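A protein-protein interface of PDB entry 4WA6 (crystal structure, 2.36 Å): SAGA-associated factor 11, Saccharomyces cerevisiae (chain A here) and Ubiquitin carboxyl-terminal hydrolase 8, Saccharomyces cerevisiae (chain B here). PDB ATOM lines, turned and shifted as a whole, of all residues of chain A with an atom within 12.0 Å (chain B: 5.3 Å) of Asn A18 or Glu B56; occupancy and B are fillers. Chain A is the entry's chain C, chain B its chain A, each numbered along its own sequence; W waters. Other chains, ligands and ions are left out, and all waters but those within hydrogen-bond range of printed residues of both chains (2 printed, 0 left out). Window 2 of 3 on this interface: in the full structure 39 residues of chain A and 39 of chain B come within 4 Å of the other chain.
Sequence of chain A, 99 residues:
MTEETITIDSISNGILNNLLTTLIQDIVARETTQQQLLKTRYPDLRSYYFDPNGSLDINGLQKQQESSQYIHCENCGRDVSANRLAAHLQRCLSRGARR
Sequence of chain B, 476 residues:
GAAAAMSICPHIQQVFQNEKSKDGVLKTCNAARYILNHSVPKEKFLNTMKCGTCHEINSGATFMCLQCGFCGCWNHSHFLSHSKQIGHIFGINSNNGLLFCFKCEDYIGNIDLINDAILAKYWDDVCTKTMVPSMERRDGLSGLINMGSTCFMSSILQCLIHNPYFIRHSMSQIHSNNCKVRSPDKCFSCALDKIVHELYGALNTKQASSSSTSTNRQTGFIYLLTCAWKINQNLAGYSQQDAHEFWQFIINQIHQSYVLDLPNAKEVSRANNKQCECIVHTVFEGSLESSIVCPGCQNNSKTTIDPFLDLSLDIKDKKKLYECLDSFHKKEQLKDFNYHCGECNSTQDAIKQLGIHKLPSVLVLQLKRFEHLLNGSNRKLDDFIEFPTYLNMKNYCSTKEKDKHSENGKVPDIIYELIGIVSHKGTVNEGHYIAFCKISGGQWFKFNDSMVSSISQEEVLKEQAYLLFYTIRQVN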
ATOM      1  N   THR A   5      -9.616   0.852  14.402  1.00  0.00           N
ATOM      2  CA  THR A   5      -8.412  -0.001  14.131  1.00  0.00           C
ATOM      3  C   THR A   5      -7.296   0.813  13.428  1.00  0.00           C
ATOM      4  O   THR A   5      -7.059   1.949  13.834  1.00  0.00           O
ATOM      5  CB  THR A   5      -8.792  -1.277  13.359  1.00  0.00           C
ATOM      6  OG1 THR A   5      -9.518  -0.905  12.168  1.00  0.00           O
ATOM      7  CG2 THR A   5      -9.618  -2.234  14.288  1.00  0.00           C
ATOM      8  N   ILE A   6      -6.593   0.271  12.424  1.00  0.00           N
ATOM      9  CA  ILE A   6      -5.395   0.964  11.958  1.00  0.00           C
ATOM     10  C   ILE A   6      -5.450   1.383  10.512  1.00  0.00           C
ATOM     11  O   ILE A   6      -5.982   0.681   9.685  1.00  0.00           O
ATOM     12  CB  ILE A   6      -4.091   0.192  12.260  1.00  0.00           C
ATOM     13  CG1 ILE A   6      -4.027  -1.162  11.547  1.00  0.00           C
ATOM     14  CG2 ILE A   6      -3.915   0.019  13.770  1.00  0.00           C
ATOM     15  CD1 ILE A   6      -2.608  -1.714  11.484  1.00  0.00           C
ATOM     16  N   THR A   7      -4.931   2.570  10.243  1.00  0.00           N
ATOM     17  CA  THR A   7      -4.889   3.131   8.924  1.00  0.00           C
ATOM     18  C   THR A   7      -3.527   3.752   8.716  1.00  0.00           C
ATOM     19  O   THR A   7      -2.712   3.832   9.636  1.00  0.00           O
ATOM     20  CB  THR A   7      -5.898   4.245   8.804  1.00  0.00           C
ATOM     21  OG1 THR A   7      -5.510   5.285   9.710  1.00  0.00           O
ATOM     22  CG2 THR A   7      -7.293   3.733   9.140  1.00  0.00           C
ATOM     23  N   ASP A   9      -2.913   6.803   8.250  1.00  0.00           N
ATOM     24  CA  ASP A   9      -2.831   8.041   9.010  1.00  0.00           C
ATOM     25  C   ASP A   9      -2.598   7.779  10.452  1.00  0.00           C
ATOM     26  O   ASP A   9      -1.750   8.388  11.038  1.00  0.00           O
ATOM     27  CB  ASP A   9      -4.078   8.855   8.878  1.00  0.00           C
ATOM     28  CG  ASP A   9      -4.229   9.407   7.519  1.00  0.00           C
ATOM     29  OD1 ASP A   9      -3.188   9.581   6.835  1.00  0.00           O
ATOM     30  OD2 ASP A   9      -5.398   9.636   7.107  1.00  0.00           O
ATOM     31  N   SER A  10      -3.342   6.850  11.018  1.00  0.00           N
ATOM     32  CA  SER A  10      -3.227   6.614  12.420  1.00  0.00           C
ATOM     33  C   SER A  10      -1.829   6.104  12.736  1.00  0.00           C
ATOM     34  O   SER A  10      -1.219   6.615  13.657  1.00  0.00           O
ATOM     35  CB  SER A  10      -4.306   5.662  12.910  1.00  0.00           C
ATOM     36  OG  SER A  10      -3.940   4.323  12.651  1.00  0.00           O
ATOM     37  N   ILE A  11      -1.309   5.153  11.954  1.00  0.00           N
ATOM     38  CA  ILE A  11       0.035   4.594  12.181  1.00  0.00           C
ATOM     39  C   ILE A  11       1.148   5.610  11.976  1.00  0.00           C
ATOM     40  O   ILE A  11       2.069   5.693  12.769  1.00  0.00           O
ATOM     41  CB  ILE A  11       0.327   3.374  11.277  1.00  0.00           C
ATOM     42  CG1 ILE A  11      -0.597   2.223  11.589  1.00  0.00           C
ATOM     43  CG2 ILE A  11       1.762   2.891  11.401  1.00  0.00           C
ATOM     44  CD1 ILE A  11      -0.327   1.547  12.890  1.00  0.00           C
ATOM     45  N   SER A  12       1.082   6.374  10.903  1.00  0.00           N
ATOM     46  CA  SER A  12       2.045   7.465  10.703  1.00  0.00           C
ATOM     47  C   SER A  12       2.148   8.384  11.893  1.00  0.00           C
ATOM     48  O   SER A  12       3.233   8.764  12.318  1.00  0.00           O
ATOM     49  CB  SER A  12       1.603   8.338   9.553  1.00  0.00           C
ATOM     50  OG  SER A  12       1.058   7.526   8.550  1.00  0.00           O
ATOM     51  N   ASN A  13       0.989   8.815  12.374  1.00  0.00           N
ATOM     52  CA  ASN A  13       0.921   9.747  13.471  1.00  0.00           C
ATOM     53  C   ASN A  13       1.419   9.091  14.748  1.00  0.00           C
ATOM     54  O   ASN A  13       2.059   9.766  15.574  1.00  0.00           O
ATOM     55  CB  ASN A  13      -0.509  10.228  13.660  1.00  0.00           C
ATOM     56  CG  ASN A  13      -0.928  11.238  12.621  1.00  0.00           C
ATOM     57  OD1 ASN A  13      -0.286  12.260  12.398  1.00  0.00           O
ATOM     58  ND2 ASN A  13      -2.020  10.971  12.006  1.00  0.00           N
ATOM     59  N   GLY A  14       1.146   7.786  14.884  1.00  0.00           N
ATOM     60  CA  GLY A  14       1.648   7.019  15.991  1.00  0.00           C
ATOM     61  C   GLY A  14       3.160   7.074  15.990  1.00  0.00           C
ATOM     62  O   GLY A  14       3.772   7.370  17.028  1.00  0.00           O
ATOM     63  N   ILE A  15       3.767   6.855  14.822  1.00  0.00           N
ATOM     64  CA  ILE A  15       5.190   6.815  14.738  1.00  0.00           C
ATOM     65  C   ILE A  15       5.820   8.163  15.048  1.00  0.00           C
ATOM     66  O   ILE A  15       6.742   8.267  15.870  1.00  0.00           O
ATOM     67  CB  ILE A  15       5.632   6.306  13.374  1.00  0.00           C
ATOM     68  CG1 ILE A  15       5.350   4.824  13.309  1.00  0.00           C
ATOM     69  CG2 ILE A  15       7.114   6.565  13.134  1.00  0.00           C
ATOM     70  CD1 ILE A  15       5.247   4.319  11.898  1.00  0.00           C
ATOM     71  N   LEU A  16       5.330   9.208  14.413  1.00  0.00           N
ATOM     72  CA  LEU A  16       5.825  10.567  14.691  1.00  0.00           C
ATOM     73  C   LEU A  16       5.759  10.933  16.183  1.00  0.00           C
ATOM     74  O   LEU A  16       6.722  11.473  16.770  1.00  0.00           O
ATOM     75  CB  LEU A  16       5.018  11.568  13.891  1.00  0.00           C
ATOM     76  CG  LEU A  16       5.386  13.016  14.128  1.00  0.00           C
ATOM     77  CD1 LEU A  16       6.870  13.196  13.981  1.00  0.00           C
ATOM     78  CD2 LEU A  16       4.677  13.876  13.117  1.00  0.00           C
ATOM     79  N   ASN A  17       4.645  10.581  16.807  1.00  0.00           N
ATOM     80  CA  ASN A  17       4.420  10.931  18.203  1.00  0.00           C
ATOM     81  C   ASN A  17       5.354  10.123  19.123  1.00  0.00           C
ATOM     82  O   ASN A  17       5.871  10.639  20.122  1.00  0.00           O
ATOM     83  CB  ASN A  17       2.951  10.702  18.552  1.00  0.00           C
ATOM     84  CG  ASN A  17       2.645  11.058  19.990  1.00  0.00           C
ATOM     85  OD1 ASN A  17       2.446  12.217  20.312  1.00  0.00           O
ATOM     86  ND2 ASN A  17       2.607  10.074  20.862  1.00  0.00           N
ATOM     87  N   ASN A  18       5.566   8.864  18.766  1.00  0.00           N
ATOM     88  CA  ASN A  18       6.576   8.035  19.402  1.00  0.00           C
ATOM     89  C   ASN A  18       7.934   8.705  19.315  1.00  0.00           C
ATOM     90  O   ASN A  18       8.575   8.850  20.334  1.00  0.00           O
ATOM     91  CB  ASN A  18       6.671   6.625  18.787  1.00  0.00           C
ATOM     92  CG  ASN A  18       5.570   5.671  19.287  1.00  0.00           C
ATOM     93  OD1 ASN A  18       4.622   6.056  19.888  1.00  0.00           O
ATOM     94  ND2 ASN A  18       5.711   4.410  18.974  1.00  0.00           N
ATOM     95  N   LEU A  19       8.332   9.153  18.116  1.00  0.00           N
ATOM     96  CA  LEU A  19       9.646   9.799  17.961  1.00  0.00           C
ATOM     97  C   LEU A  19       9.682  11.091  18.739  1.00  0.00           C
ATOM     98  O   LEU A  19      10.611  11.289  19.517  1.00  0.00           O
ATOM     99  CB  LEU A  19      10.015  10.097  16.515  1.00  0.00           C
ATOM    100  CG  LEU A  19      10.183   8.930  15.545  1.00  0.00           C
ATOM    101  CD1 LEU A  19      10.207   9.386  14.096  1.00  0.00           C
ATOM    102  CD2 LEU A  19      11.451   8.222  15.883  1.00  0.00           C
ATOM    103  N   LEU A  20       8.685  11.957  18.589  1.00  0.00           N
ATOM    104  CA  LEU A  20       8.737  13.259  19.303  1.00  0.00           C
ATOM    105  C   LEU A  20       8.791  13.117  20.807  1.00  0.00           C
ATOM    106  O   LEU A  20       9.543  13.812  21.447  1.00  0.00           O
ATOM    107  CB  LEU A  20       7.560  14.138  18.911  1.00  0.00           C
ATOM    108  CG  LEU A  20       7.669  14.662  17.484  1.00  0.00           C
ATOM    109  CD1 LEU A  20       6.338  15.261  16.996  1.00  0.00           C
ATOM    110  CD2 LEU A  20       8.819  15.685  17.480  1.00  0.00           C
ATOM    111  N   THR A  21       8.001  12.194  21.357  1.00  0.00           N
ATOM    112  CA  THR A  21       7.870  12.069  22.821  1.00  0.00           C
ATOM    113  C   THR A  21       9.124  11.418  23.401  1.00  0.00           C
ATOM    114  O   THR A  21       9.605  11.783  24.494  1.00  0.00           O
ATOM    115  CB  THR A  21       6.656  11.210  23.240  1.00  0.00           C
ATOM    116  OG1 THR A  21       6.641  10.007  22.435  1.00  0.00           O
ATOM    117  CG2 THR A  21       5.402  11.961  23.056  1.00  0.00           C
ATOM    118  N   THR A  22       9.645  10.443  22.674  1.00  0.00           N
ATOM    119  CA  THR A  22      10.904   9.875  23.052  1.00  0.00           C
ATOM    120  C   THR A  22      11.978  10.988  23.156  1.00  0.00           C
ATOM    121  O   THR A  22      12.640  11.155  24.245  1.00  0.00           O
ATOM    122  CB  THR A  22      11.273   8.759  22.091  1.00  0.00           C
ATOM    123  OG1 THR A  22      10.258   7.737  22.191  1.00  0.00           O
ATOM    124  CG2 THR A  22      12.665   8.221  22.406  1.00  0.00           C
ATOM    125  N   LEU A  23      12.087  11.781  22.083  1.00  0.00           N
ATOM    126  CA  LEU A  23      13.048  12.910  22.037  1.00  0.00           C
ATOM    127  C   LEU A  23      12.790  13.909  23.175  1.00  0.00           C
ATOM    128  O   LEU A  23      13.724  14.221  23.946  1.00  0.00           O
ATOM    129  CB  LEU A  23      13.013  13.625  20.693  1.00  0.00           C
ATOM    130  CG  LEU A  23      14.036  14.775  20.530  1.00  0.00           C
ATOM    131  CD1 LEU A  23      15.505  14.411  20.851  1.00  0.00           C
ATOM    132  CD2 LEU A  23      13.909  15.299  19.106  1.00  0.00           C
ATOM    133  N   ILE A  24      11.533  14.348  23.333  1.00  0.00           N
ATOM    134  CA  ILE A  24      11.202  15.274  24.406  1.00  0.00           C
ATOM    135  C   ILE A  24      11.532  14.724  25.795  1.00  0.00           C
ATOM    136  O   ILE A  24      12.011  15.440  26.645  1.00  0.00           O
ATOM    137  CB  ILE A  24       9.717  15.619  24.424  1.00  0.00           C
ATOM    138  CG1 ILE A  24       9.371  16.415  23.196  1.00  0.00           C
ATOM    139  CG2 ILE A  24       9.338  16.448  25.689  1.00  0.00           C
ATOM    140  CD1 ILE A  24       7.890  16.416  22.861  1.00  0.00           C
ATOM    141  N   GLN A  25      11.223  13.465  26.034  1.00  0.00           N
ATOM    142  CA  GLN A  25      11.491  12.855  27.306  1.00  0.00           C
ATOM    143  C   GLN A  25      12.946  12.797  27.637  1.00  0.00           C
ATOM    144  O   GLN A  25      13.368  12.867  28.822  1.00  0.00           O
ATOM    145  CB  GLN A  25      10.859  11.467  27.388  1.00  0.00           C
ATOM    146  CG  GLN A  25       9.353  11.588  27.569  1.00  0.00           C
ATOM    147  CD  GLN A  25       8.566  10.342  27.216  1.00  0.00           C
ATOM    148  OE1 GLN A  25       8.968   9.239  27.535  1.00  0.00           O
ATOM    149  NE2 GLN A  25       7.407  10.531  26.587  1.00  0.00           N
ATOM    150  N   ASP A  26      13.707  12.639  26.608  1.00  0.00           N
ATOM    151  CA  ASP A  26      15.146  12.497  26.725  1.00  0.00           C
ATOM    152  C   ASP A  26      15.722  13.863  27.075  1.00  0.00           C
ATOM    153  O   ASP A  26      16.501  13.967  27.976  1.00  0.00           O
ATOM    154  CB  ASP A  26      15.730  12.021  25.385  1.00  0.00           C
ATOM    155  CG  ASP A  26      17.254  11.856  25.418  1.00  0.00           C
ATOM    156  OD1 ASP A  26      17.922  11.706  26.506  1.00  0.00           O
ATOM    157  OD2 ASP A  26      17.816  11.894  24.314  1.00  0.00           O
ATOM    158  N   ILE A  27      15.354  14.898  26.323  1.00  0.00           N
ATOM    159  CA  ILE A  27      15.816  16.240  26.612  1.00  0.00           C
ATOM    160  C   ILE A  27      15.386  16.618  28.037  1.00  0.00           C
ATOM    161  O   ILE A  27      16.180  17.218  28.784  1.00  0.00           O
ATOM    162  CB  ILE A  27      15.253  17.246  25.584  1.00  0.00           C
ATOM    163  CG1 ILE A  27      15.896  17.074  24.197  1.00  0.00           C
ATOM    164  CG2 ILE A  27      15.391  18.692  26.005  1.00  0.00           C
ATOM    165  CD1 ILE A  27      14.997  17.676  23.137  1.00  0.00           C
ATOM    166  N   MET B  49      14.880  -0.508  22.569  1.00  0.00           N
ATOM    167  CA  MET B  49      13.868   0.528  22.420  1.00  0.00           C
ATOM    168  C   MET B  49      12.516  -0.026  22.102  1.00  0.00           C
ATOM    169  O   MET B  49      11.641   0.675  21.648  1.00  0.00           O
ATOM    170  CB  MET B  49      14.355   1.556  21.399  1.00  0.00           C
ATOM    171  CG  MET B  49      15.419   2.447  22.054  1.00  0.00           C
ATOM    172  SD  MET B  49      16.155   3.618  20.917  1.00  0.00           S
ATOM    173  CE  MET B  49      17.289   4.424  22.051  1.00  0.00           C
ATOM    174  N   LYS B  50      12.340  -1.306  22.397  1.00  0.00           N
ATOM    175  CA  LYS B  50      11.101  -1.963  22.123  1.00  0.00           C
ATOM    176  C   LYS B  50      10.473  -2.434  23.412  1.00  0.00           C
ATOM    177  O   LYS B  50      11.086  -3.151  24.165  1.00  0.00           O
ATOM    178  CB  LYS B  50      11.356  -3.151  21.215  1.00  0.00           C
ATOM    179  CG  LYS B  50      10.065  -3.767  20.709  1.00  0.00           C
ATOM    180  CD  LYS B  50      10.207  -5.246  20.531  1.00  0.00           C
ATOM    181  CE  LYS B  50      10.784  -5.589  19.192  1.00  0.00           C
ATOM    182  NZ  LYS B  50      10.371  -6.995  18.929  1.00  0.00           N
ATOM    183  N   CYS B  51       9.220  -2.057  23.642  1.00  0.00           N
ATOM    184  CA  CYS B  51       8.528  -2.457  24.823  1.00  0.00           C
ATOM    185  C   CYS B  51       8.187  -3.934  24.845  1.00  0.00           C
ATOM    186  O   CYS B  51       7.602  -4.466  23.911  1.00  0.00           O
ATOM    187  CB  CYS B  51       7.245  -1.663  24.959  1.00  0.00           C
ATOM    188  SG  CYS B  51       6.398  -1.953  26.527  1.00  0.00           S
ATOM    189  N   CYS B  54       3.980  -3.984  24.870  1.00  0.00           N
ATOM    190  CA  CYS B  54       3.176  -3.621  23.688  1.00  0.00           C
ATOM    191  C   CYS B  54       3.956  -3.805  22.412  1.00  0.00           C
ATOM    192  O   CYS B  54       3.392  -3.671  21.366  1.00  0.00           O
ATOM    193  CB  CYS B  54       2.687  -2.156  23.783  1.00  0.00           C
ATOM    194  SG  CYS B  54       4.028  -0.940  23.961  1.00  0.00           S
ATOM    195  N   HIS B  55       5.255  -4.033  22.508  1.00  0.00           N
ATOM    196  CA  HIS B  55       6.132  -4.241  21.334  1.00  0.00           C
ATOM    197  C   HIS B  55       6.292  -3.054  20.385  1.00  0.00           C
ATOM    198  O   HIS B  55       6.838  -3.202  19.327  1.00  0.00           O
ATOM    199  CB  HIS B  55       5.750  -5.492  20.526  1.00  0.00           C
ATOM    200  CG  HIS B  55       5.585  -6.708  21.353  1.00  0.00           C
ATOM    201  ND1 HIS B  55       6.629  -7.272  22.048  1.00  0.00           N
ATOM    202  CD2 HIS B  55       4.490  -7.453  21.635  1.00  0.00           C
ATOM    203  CE1 HIS B  55       6.186  -8.311  22.732  1.00  0.00           C
ATOM    204  NE2 HIS B  55       4.892  -8.444  22.496  1.00  0.00           N
ATOM    205  N   GLU B  56       5.872  -1.869  20.778  1.00  0.00           N
ATOM    206  CA  GLU B  56       6.141  -0.686  19.977  1.00  0.00           C
ATOM    207  C   GLU B  56       7.566  -0.234  20.187  1.00  0.00           C
ATOM    208  O   GLU B  56       8.092  -0.369  21.273  1.00  0.00           O
ATOM    209  CB  GLU B  56       5.206   0.458  20.339  1.00  0.00           C
ATOM    210  CG  GLU B  56       3.730   0.167  20.114  1.00  0.00           C
ATOM    211  CD  GLU B  56       2.899   1.434  20.074  1.00  0.00           C
ATOM    212  OE1 GLU B  56       1.882   1.516  20.807  1.00  0.00           O
ATOM    213  OE2 GLU B  56       3.268   2.347  19.293  1.00  0.00           O
ATOM    214  N   ILE B  57       8.164   0.308  19.125  1.00  0.00           N
ATOM    215  CA  ILE B  57       9.432   0.988  19.187  1.00  0.00           C
ATOM    216  C   ILE B  57       9.262   2.463  19.605  1.00  0.00           C
ATOM    217  O   ILE B  57       8.420   3.156  19.061  1.00  0.00           O
ATOM    218  CB  ILE B  57      10.115   0.962  17.828  1.00  0.00           C
ATOM    219  CG1 ILE B  57      10.077  -0.459  17.218  1.00  0.00           C
ATOM    220  CG2 ILE B  57      11.542   1.414  17.985  1.00  0.00           C
ATOM    221  CD1 ILE B  57      10.881  -1.472  17.979  1.00  0.00           C
ATOM    222  N   ASN B  58      10.080   2.940  20.548  1.00  0.00           N
ATOM    223  CA  ASN B  58      10.036   4.317  21.010  1.00  0.00           C
ATOM    224  C   ASN B  58       8.660   4.790  21.457  1.00  0.00           C
ATOM    225  O   ASN B  58       8.202   5.844  21.011  1.00  0.00           O
ATOM    226  CB  ASN B  58      10.550   5.264  19.896  1.00  0.00           C
ATOM    227  CG  ASN B  58      12.037   5.123  19.623  1.00  0.00           C
ATOM    228  OD1 ASN B  58      12.851   4.896  20.520  1.00  0.00           O
ATOM    229  ND2 ASN B  58      12.401   5.294  18.395  1.00  0.00           N
ATOM    230  N   SER B  59       7.985   4.040  22.338  1.00  0.00           N
ATOM    231  CA  SER B  59       6.686   4.481  22.976  1.00  0.00           C
ATOM    232  C   SER B  59       7.018   5.363  24.187  1.00  0.00           C
ATOM    233  O   SER B  59       6.856   5.017  25.398  1.00  0.00           O
ATOM    234  CB  SER B  59       5.891   3.277  23.379  1.00  0.00           C
ATOM    235  OG  SER B  59       4.610   3.642  23.839  1.00  0.00           O
ATOM    236  N   GLY B  60       7.550   6.524  23.824  1.00  0.00           N
ATOM    237  CA  GLY B  60       8.287   7.324  24.734  1.00  0.00           C
ATOM    238  C   GLY B  60       9.575   6.594  25.035  1.00  0.00           C
ATOM    239  O   GLY B  60       9.977   5.635  24.323  1.00  0.00           O
ATOM    240  N   ASN B  75       5.168   5.704  27.594  1.00  0.00           N
ATOM    241  CA  ASN B  75       3.867   6.191  27.184  1.00  0.00           C
ATOM    242  C   ASN B  75       2.642   5.371  27.633  1.00  0.00           C
ATOM    243  O   ASN B  75       1.581   5.929  27.812  1.00  0.00           O
ATOM    244  CB  ASN B  75       3.852   6.452  25.675  1.00  0.00           C
ATOM    245  CG  ASN B  75       4.694   7.666  25.290  1.00  0.00           C
ATOM    246  OD1 ASN B  75       5.388   8.230  26.095  1.00  0.00           O
ATOM    247  ND2 ASN B  75       4.652   8.044  24.085  1.00  0.00           N
ATOM    248  N   HIS B  76       2.760   4.057  27.744  1.00  0.00           N
ATOM    249  CA  HIS B  76       1.643   3.248  28.183  1.00  0.00           C
ATOM    250  C   HIS B  76       1.902   2.687  29.585  1.00  0.00           C
ATOM    251  O   HIS B  76       1.214   1.774  29.996  1.00  0.00           O
ATOM    252  CB  HIS B  76       1.326   2.119  27.205  1.00  0.00           C
ATOM    253  CG  HIS B  76       0.992   2.590  25.827  1.00  0.00           C
ATOM    254  ND1 HIS B  76       1.782   2.291  24.733  1.00  0.00           N
ATOM    255  CD2 HIS B  76      -0.032   3.345  25.361  1.00  0.00           C
ATOM    256  CE1 HIS B  76       1.274   2.869  23.658  1.00  0.00           C
ATOM    257  NE2 HIS B  76       0.179   3.523  24.015  1.00  0.00           N
HETATM  258  O   HOH W   1       1.973   4.559  17.935  1.00  0.00           O
HETATM  259  O   HOH W   2       7.725   3.782  16.480  1.00  0.00           O
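Asn A18 touches just these residues of chain B: Glu B56, Ile B57 and Asn B58.
Of the printed residues of chain B, Leu A19 touches Asn B58 (3.97 Å).
Of the printed residues of chain B, Thr A21 touches Gly B60 (3.9 Å) and Asn B75 (3.2 Å).
Of the printed residues of chain B, Thr A22 touches Asn B58 and Gly B60.
Printed residues of chain B within 4 Å of Gln A25: Gly B60 and Asn B75.
No residue of chain A comes within 4 Å of Lys B50.
No residue of chain A comes within 4 Å of Cys B51.
No residue of chain A comes within 4 Å of His B55.
Glu B56 touches just one residue of chain A: Asn A18 (3.2 Å).
Of chain A, only Asn A18 (3.0 Å) comes within 4 Å of Ile B57.
Asn B58 touches three residues of chain A.
No residue of chain A comes within 4 Å of Ser B59.
Of the printed residues of chain A, Gly B60 touches Thr A21, Thr A22 and Gln A25.
Printed residues of chain A within 4 Å of Asn B75: Thr A21 (3.2 Å) and Gln A25 (3.1 Å).
His B76 touches none of the printed residues of chain A.
Among the printed residues, pairs that only touch across the chains: Gln A25 with Gly B60 (3.5 Å), Thr A21 with Gly B60 (3.9 Å) and Leu A19 with Asn B58 (3.97 Å).
Water W2 lies within hydrogen-bond range of the backbone carbonyl oxygen (O) of Ile B57 (2.7 Å) and the side-chain amide nitrogen (ND2) of Asn A18 (3.3 Å).
Water W1 lies within hydrogen-bond range of the side-chain carboxylate of Glu B56 and the backbone carbonyl oxygen of Gly A14.
The backbone NH (N) of Asn B58 is in hydrogen-bond range of the backbone carbonyl oxygen (O) of Met B49 (3.0 Å).
The backbone NH of Cys B51 is in hydrogen-bond range of the backbone carbonyl oxygen of Glu B56, 3.1 Å away.
The side-chain amide nitrogen (ND2) of Asn B75 lies close to the backbone NH (N) of Gly B60 (3.3 Å).
The backbone carbonyl oxygen (O) of Gly A14 sits close to the side-chain amide oxygen (OD1) of Asn A18 (3.3 Å).
The side-chain hydroxyl of Thr A21 lies within hydrogen-bond range of the backbone carbonyl oxygen of Asn A17 (2.5 Å).
OG1 of Thr A22 is in hydrogen-bond range of O of Asn A18, 2.7 Å away.
The side-chain amide nitrogen of Asn A18 is in hydrogen-bond range of the side-chain carboxylate of Glu B56.
O of Ile B57 sits at hydrogen-bond distance from ND2 of Asn A18 (3.0 Å).
OG1 of Thr A22 is in hydrogen-bond range of O of Asn B58 (3.0 Å).
The side-chain hydroxyl (OG1) of Thr A22 lies within hydrogen-bond range of the backbone carbonyl oxygen (O) of Gly B60 (3.0 Å).
The side-chain amide nitrogen of Asn B75 lies within hydrogen-bond range of the side-chain hydroxyl of Thr A21.
The side-chain amide nitrogen (NE2) of Gln A25 lies within hydrogen-bond range of the side-chain amide oxygen (OD1) of Asn B75.
The backbone carbonyl oxygen of Asn A18 lies close to the backbone carbonyl oxygen of Asn B58, at 3.1 Å.
Printed residues of chain A that touch a printed residue of chain B: Asn A18, Leu A19, Thr A21, Thr A22 and Gln A25.
Hydrophobic or aromatic side chains of chain A within 4 Å of the printed part of chain B: Leu A19.
Of the 12 printed residues of chain B, 5 touch a printed residue of chain A.
Along chain B the printed residues that touch a printed residue of chain A span positions 56 to 75.
Among the printed residues, 10 pairs touch across the chains.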
